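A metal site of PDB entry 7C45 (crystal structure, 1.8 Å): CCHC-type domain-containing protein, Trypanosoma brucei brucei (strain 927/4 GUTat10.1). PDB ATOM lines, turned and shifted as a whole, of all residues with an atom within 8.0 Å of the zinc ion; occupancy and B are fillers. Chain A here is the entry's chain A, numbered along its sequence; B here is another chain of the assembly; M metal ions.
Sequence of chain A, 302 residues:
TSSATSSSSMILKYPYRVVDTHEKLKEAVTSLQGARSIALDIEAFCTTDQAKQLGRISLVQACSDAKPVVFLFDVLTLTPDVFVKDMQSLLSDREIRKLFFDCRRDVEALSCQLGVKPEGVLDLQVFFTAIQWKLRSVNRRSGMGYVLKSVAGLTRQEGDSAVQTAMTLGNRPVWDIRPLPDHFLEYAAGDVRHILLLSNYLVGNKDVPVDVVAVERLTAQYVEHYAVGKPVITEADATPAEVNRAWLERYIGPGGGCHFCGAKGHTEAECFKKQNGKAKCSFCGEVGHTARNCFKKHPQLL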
ATOM      1  N   GLY A 257      -3.378  20.871 -14.170  1.00  0.00           N
ATOM      2  CA  GLY A 257      -2.569  19.679 -14.142  1.00  0.00           C
ATOM      3  C   GLY A 257      -3.436  18.439 -14.013  1.00  0.00           C
ATOM      4  O   GLY A 257      -4.664  18.503 -14.024  1.00  0.00           O
ATOM      5  N   CYS A 258      -2.769  17.306 -13.883  1.00  0.00           N
ATOM      6  CA  CYS A 258      -3.459  16.027 -13.907  1.00  0.00           C
ATOM      7  C   CYS A 258      -4.166  15.807 -12.567  1.00  0.00           C
ATOM      8  O   CYS A 258      -3.534  15.807 -11.513  1.00  0.00           O
ATOM      9  CB  CYS A 258      -2.476  14.898 -14.185  1.00  0.00           C
ATOM     10  SG  CYS A 258      -3.235  13.267 -14.071  1.00  0.00           S
ATOM     11  N   HIS A 259      -5.483  15.653 -12.613  1.00  0.00           N
ATOM     12  CA  HIS A 259      -6.209  15.423 -11.362  1.00  0.00           C
ATOM     13  C   HIS A 259      -5.826  14.111 -10.694  1.00  0.00           C
ATOM     14  O   HIS A 259      -6.074  13.951  -9.492  1.00  0.00           O
ATOM     15  CB  HIS A 259      -7.708  15.413 -11.625  1.00  0.00           C
ATOM     16  CG  HIS A 259      -8.269  16.751 -11.990  1.00  0.00           C
ATOM     17  ND1 HIS A 259      -9.604  16.963 -12.240  1.00  0.00           N
ATOM     18  CD2 HIS A 259      -7.661  17.953 -12.156  1.00  0.00           C
ATOM     19  CE1 HIS A 259      -9.803  18.233 -12.544  1.00  0.00           C
ATOM     20  NE2 HIS A 259      -8.644  18.857 -12.497  1.00  0.00           N
ATOM     21  N   PHE A 260      -5.283  13.145 -11.442  1.00  0.00           N
ATOM     22  CA  PHE A 260      -5.033  11.829 -10.854  1.00  0.00           C
ATOM     23  C   PHE A 260      -3.703  11.769 -10.122  1.00  0.00           C
ATOM     24  O   PHE A 260      -3.620  11.205  -9.026  1.00  0.00           O
ATOM     25  CB  PHE A 260      -5.078  10.736 -11.937  1.00  0.00           C
ATOM     26  CG  PHE A 260      -4.938   9.323 -11.372  1.00  0.00           C
ATOM     27  CD1 PHE A 260      -6.052   8.642 -10.899  1.00  0.00           C
ATOM     28  CD2 PHE A 260      -3.698   8.717 -11.292  1.00  0.00           C
ATOM     29  CE1 PHE A 260      -5.924   7.384 -10.386  1.00  0.00           C
ATOM     30  CE2 PHE A 260      -3.568   7.459 -10.797  1.00  0.00           C
ATOM     31  CZ  PHE A 260      -4.683   6.786 -10.335  1.00  0.00           C
ATOM     32  N   CYS A 261      -2.644  12.316 -10.724  1.00  0.00           N
ATOM     33  CA  CYS A 261      -1.314  12.262 -10.132  1.00  0.00           C
ATOM     34  C   CYS A 261      -0.761  13.622  -9.774  1.00  0.00           C
ATOM     35  O   CYS A 261       0.273  13.685  -9.134  1.00  0.00           O
ATOM     36  CB  CYS A 261      -0.316  11.582 -11.078  1.00  0.00           C
ATOM     37  SG  CYS A 261       0.212  12.610 -12.485  1.00  0.00           S
ATOM     38  N   GLY A 262      -1.414  14.704 -10.197  1.00  0.00           N
ATOM     39  CA  GLY A 262      -0.978  16.028  -9.807  1.00  0.00           C
ATOM     40  C   GLY A 262       0.091  16.658 -10.677  1.00  0.00           C
ATOM     41  O   GLY A 262       0.431  17.822 -10.453  1.00  0.00           O
ATOM     42  N   ALA A 263       0.633  15.931 -11.654  1.00  0.00           N
ATOM     43  CA  ALA A 263       1.708  16.479 -12.474  1.00  0.00           C
ATOM     44  C   ALA A 263       1.160  17.479 -13.489  1.00  0.00           C
ATOM     45  O   ALA A 263       0.028  17.354 -13.973  1.00  0.00           O
ATOM     46  CB  ALA A 263       2.447  15.370 -13.226  1.00  0.00           C
ATOM     47  N   LYS A 264       1.967  18.485 -13.784  1.00  0.00           N
ATOM     48  CA  LYS A 264       1.662  19.358 -14.896  1.00  0.00           C
ATOM     49  C   LYS A 264       2.050  18.659 -16.199  1.00  0.00           C
ATOM     50  O   LYS A 264       2.846  17.726 -16.209  1.00  0.00           O
ATOM     51  CB  LYS A 264       2.388  20.696 -14.697  1.00  0.00           C
ATOM     52  CG  LYS A 264       1.661  21.578 -13.712  1.00  0.00           C
ATOM     53  CD  LYS A 264       2.559  22.377 -12.822  1.00  0.00           C
ATOM     54  CE  LYS A 264       1.750  22.874 -11.617  1.00  0.00           C
ATOM     55  NZ  LYS A 264       1.464  24.344 -11.628  1.00  0.00           N
ATOM     56  N   GLY A 265       1.442  19.097 -17.300  1.00  0.00           N
ATOM     57  CA  GLY A 265       1.820  18.611 -18.610  1.00  0.00           C
ATOM     58  C   GLY A 265       0.848  17.644 -19.229  1.00  0.00           C
ATOM     59  O   GLY A 265       0.939  17.384 -20.442  1.00  0.00           O
ATOM     60  N   HIS A 266      -0.089  17.090 -18.460  1.00  0.00           N
ATOM     61  CA  HIS A 266      -1.087  16.203 -19.043  1.00  0.00           C
ATOM     62  C   HIS A 266      -2.331  16.221 -18.167  1.00  0.00           C
ATOM     63  O   HIS A 266      -2.346  16.782 -17.066  1.00  0.00           O
ATOM     64  CB  HIS A 266      -0.569  14.783 -19.177  1.00  0.00           C
ATOM     65  CG  HIS A 266      -0.308  14.112 -17.866  1.00  0.00           C
ATOM     66  ND1 HIS A 266       0.926  14.082 -17.265  1.00  0.00           N
ATOM     67  CD2 HIS A 266      -1.143  13.402 -17.055  1.00  0.00           C
ATOM     68  CE1 HIS A 266       0.846  13.407 -16.120  1.00  0.00           C
ATOM     69  NE2 HIS A 266      -0.401  12.989 -15.979  1.00  0.00           N
ATOM     70  N   THR A 267      -3.397  15.599 -18.676  1.00  0.00           N
ATOM     71  CA  THR A 267      -4.649  15.508 -17.959  1.00  0.00           C
ATOM     72  C   THR A 267      -4.899  14.074 -17.525  1.00  0.00           C
ATOM     73  O   THR A 267      -4.258  13.131 -17.993  1.00  0.00           O
ATOM     74  CB  THR A 267      -5.846  15.979 -18.791  1.00  0.00           C
ATOM     75  OG1 THR A 267      -6.100  15.026 -19.815  1.00  0.00           O
ATOM     76  CG2 THR A 267      -5.607  17.341 -19.404  1.00  0.00           C
ATOM     77  N   GLU A 268      -5.887  13.949 -16.640  1.00  0.00           N
ATOM     78  CA  GLU A 268      -6.280  12.653 -16.111  1.00  0.00           C
ATOM     79  C   GLU A 268      -6.558  11.654 -17.228  1.00  0.00           C
ATOM     80  O   GLU A 268      -6.177  10.497 -17.132  1.00  0.00           O
ATOM     81  CB  GLU A 268      -7.514  12.837 -15.216  1.00  0.00           C
ATOM     82  CG  GLU A 268      -8.234  11.577 -14.814  1.00  0.00           C
ATOM     83  CD  GLU A 268      -9.550  11.867 -14.120  1.00  0.00           C
ATOM     84  OE1 GLU A 268      -9.536  12.515 -13.060  1.00  0.00           O
ATOM     85  OE2 GLU A 268     -10.608  11.475 -14.653  1.00  0.00           O
ATOM     86  N   ALA A 269      -7.203  12.117 -18.310  1.00  0.00           N
ATOM     87  CA  ALA A 269      -7.565  11.197 -19.384  1.00  0.00           C
ATOM     88  C   ALA A 269      -6.346  10.611 -20.094  1.00  0.00           C
ATOM     89  O   ALA A 269      -6.467   9.564 -20.738  1.00  0.00           O
ATOM     90  CB  ALA A 269      -8.433  11.905 -20.422  1.00  0.00           C
ATOM     91  N   GLU A 270      -5.197  11.274 -19.979  1.00  0.00           N
ATOM     92  CA  GLU A 270      -3.965  10.882 -20.619  1.00  0.00           C
ATOM     93  C   GLU A 270      -2.938  10.302 -19.653  1.00  0.00           C
ATOM     94  O   GLU A 270      -1.808  10.025 -20.067  1.00  0.00           O
ATOM     95  CB  GLU A 270      -3.325  12.086 -21.333  1.00  0.00           C
ATOM     96  CG  GLU A 270      -4.297  13.041 -22.028  1.00  0.00           C
ATOM     97  CD  GLU A 270      -3.723  14.442 -22.209  1.00  0.00           C
ATOM     98  OE1 GLU A 270      -4.073  15.109 -23.203  1.00  0.00           O
ATOM     99  OE2 GLU A 270      -2.912  14.890 -21.362  1.00  0.00           O
ATOM    100  N   CYS A 271      -3.282  10.124 -18.377  1.00  0.00           N
ATOM    101  CA  CYS A 271      -2.288   9.844 -17.336  1.00  0.00           C
ATOM    102  C   CYS A 271      -1.732   8.437 -17.433  1.00  0.00           C
ATOM    103  O   CYS A 271      -2.482   7.459 -17.320  1.00  0.00           O
ATOM    104  CB  CYS A 271      -2.932  10.061 -15.965  1.00  0.00           C
ATOM    105  SG  CYS A 271      -1.789   9.799 -14.610  1.00  0.00           S
ATOM    106  N   PHE A 272      -0.418   8.328 -17.611  1.00  0.00           N
ATOM    107  CA  PHE A 272       0.242   7.028 -17.627  1.00  0.00           C
ATOM    108  C   PHE A 272       0.085   6.315 -16.297  1.00  0.00           C
ATOM    109  O   PHE A 272       0.024   5.092 -16.253  1.00  0.00           O
ATOM    110  CB  PHE A 272       1.735   7.179 -17.955  1.00  0.00           C
ATOM    111  CG  PHE A 272       2.029   7.755 -19.310  1.00  0.00           C
ATOM    112  CD1 PHE A 272       1.191   7.508 -20.380  1.00  0.00           C
ATOM    113  CD2 PHE A 272       3.145   8.562 -19.504  1.00  0.00           C
ATOM    114  CE1 PHE A 272       1.462   8.062 -21.638  1.00  0.00           C
ATOM    115  CE2 PHE A 272       3.425   9.107 -20.743  1.00  0.00           C
ATOM    116  CZ  PHE A 272       2.583   8.846 -21.813  1.00  0.00           C
ATOM    117  N   LYS A 273       0.068   7.059 -15.191  1.00  0.00           N
ATOM    118  CA  LYS A 273      -0.035   6.398 -13.892  1.00  0.00           C
ATOM    119  C   LYS A 273      -1.420   5.804 -13.687  1.00  0.00           C
ATOM    120  O   LYS A 273      -1.548   4.660 -13.251  1.00  0.00           O
ATOM    121  CB  LYS A 273       0.332   7.368 -12.779  1.00  0.00           C
ATOM    122  CG  LYS A 273       1.791   7.865 -12.894  1.00  0.00           C
ATOM    123  CD  LYS A 273       2.236   8.496 -11.607  1.00  0.00           C
ATOM    124  CE  LYS A 273       3.740   8.801 -11.580  1.00  0.00           C
ATOM    125  NZ  LYS A 273       4.023   9.885 -10.569  1.00  0.00           N
ATOM    126  N   LYS A 274      -2.477   6.536 -14.052  1.00  0.00           N
ATOM    127  CA  LYS A 274      -3.822   5.997 -13.908  1.00  0.00           C
ATOM    128  C   LYS A 274      -4.031   4.815 -14.829  1.00  0.00           C
ATOM    129  O   LYS A 274      -4.713   3.844 -14.467  1.00  0.00           O
ATOM    130  CB  LYS A 274      -4.858   7.089 -14.166  1.00  0.00           C
ATOM    131  CG  LYS A 274      -6.302   6.617 -14.155  1.00  0.00           C
ATOM    132  CD  LYS A 274      -7.257   7.732 -14.500  1.00  0.00           C
ATOM    133  CE  LYS A 274      -8.709   7.359 -14.173  1.00  0.00           C
ATOM    134  NZ  LYS A 274      -9.580   8.453 -14.574  1.00  0.00           N
ATOM    135  N   GLN A 275      -3.426   4.865 -16.020  1.00  0.00           N
ATOM    136  CA  GLN A 275      -3.537   3.761 -16.970  1.00  0.00           C
ATOM    137  C   GLN A 275      -2.674   2.589 -16.550  1.00  0.00           C
ATOM    138  O   GLN A 275      -2.974   1.451 -16.905  1.00  0.00           O
ATOM    139  CB  GLN A 275      -3.135   4.230 -18.371  1.00  0.00           C
ATOM    140  CG  GLN A 275      -4.024   5.341 -18.901  1.00  0.00           C
ATOM    141  CD  GLN A 275      -3.408   6.131 -20.057  1.00  0.00           C
ATOM    142  OE1 GLN A 275      -2.355   5.769 -20.608  1.00  0.00           O
ATOM    143  NE2 GLN A 275      -4.079   7.211 -20.429  1.00  0.00           N
ATOM    144  P     U B   4       7.934  12.584 -25.230  1.00  0.00           P
ATOM    145  OP1   U B   4       8.596  13.246 -26.396  1.00  0.00           O
ATOM    146  OP2   U B   4       8.768  11.855 -24.252  1.00  0.00           O
ATOM    147  O5'   U B   4       7.019  13.628 -24.433  1.00  0.00           O
ATOM    148  C5'   U B   4       6.086  13.206 -23.431  1.00  0.00           C
ATOM    149  C4'   U B   4       4.691  13.015 -23.986  1.00  0.00           C
ATOM    150  O4'   U B   4       3.904  12.192 -23.076  1.00  0.00           O
ATOM    151  C3'   U B   4       3.869  14.280 -24.226  1.00  0.00           C
ATOM    152  O3'   U B   4       3.049  14.013 -25.370  1.00  0.00           O
ATOM    153  C2'   U B   4       2.968  14.319 -22.980  1.00  0.00           C
ATOM    154  O2'   U B   4       1.772  15.051 -23.154  1.00  0.00           O
ATOM    155  C1'   U B   4       2.676  12.842 -22.803  1.00  0.00           C
ATOM    156  N1    U B   4       2.224  12.384 -21.481  1.00  0.00           N
ATOM    157  C2    U B   4       0.981  11.761 -21.385  1.00  0.00           C
ATOM    158  O2    U B   4       0.207  11.659 -22.304  1.00  0.00           O
ATOM    159  N3    U B   4       0.650  11.287 -20.129  1.00  0.00           N
ATOM    160  C4    U B   4       1.432  11.360 -19.012  1.00  0.00           C
ATOM    161  O4    U B   4       1.023  10.875 -17.947  1.00  0.00           O
ATOM    162  C5    U B   4       2.703  11.990 -19.199  1.00  0.00           C
ATOM    163  C6    U B   4       3.055  12.452 -20.389  1.00  0.00           C
HETATM  164 ZN    ZN M   1      -1.261  12.054 -14.242  1.00  0.00          ZN
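ND1 of His 266 sits close to O4 of U 4 of chain B (3.3 Å). The side-chain sulfur (SG) of Cys 258 lies close to the backbone NH (N) of Phe 260 (3.3 Å). The backbone NH (N) of Cys 258 lies within hydrogen-bond range of the backbone carbonyl oxygen (O) of Ala 263 (2.8 Å). SG of Cys 258 lies close to N of Glu 268 (3.8 Å). SG of Cys 271 sits close to N of Lys 273 (3.4 Å). N of Lys 274 sits close to SG of Cys 271 (3.4 Å). The side-chain sulfur (SG) of Cys 261 sits close to the backbone NH (N) of Ala 263 (3.4 Å).
Four residues have an atom within 4 Å of the zinc ion: Cys 258, Cys 261, His 266 and Cys 271. The nearest printed residue that does not touch the zinc ion is U 4 of chain B (4.5 Å).
The zinc ion is bound by a ring nitrogen (NE2) of His 266 (2.2 Å), the side-chain sulfur (SG) of Cys 258 (2.3 Å), the side-chain sulfur (SG) of Cys 271 (2.3 Å) and the side-chain sulfur (SG) of Cys 261 (2.4 Å). The zinc ion has four donor atoms within binding distance.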
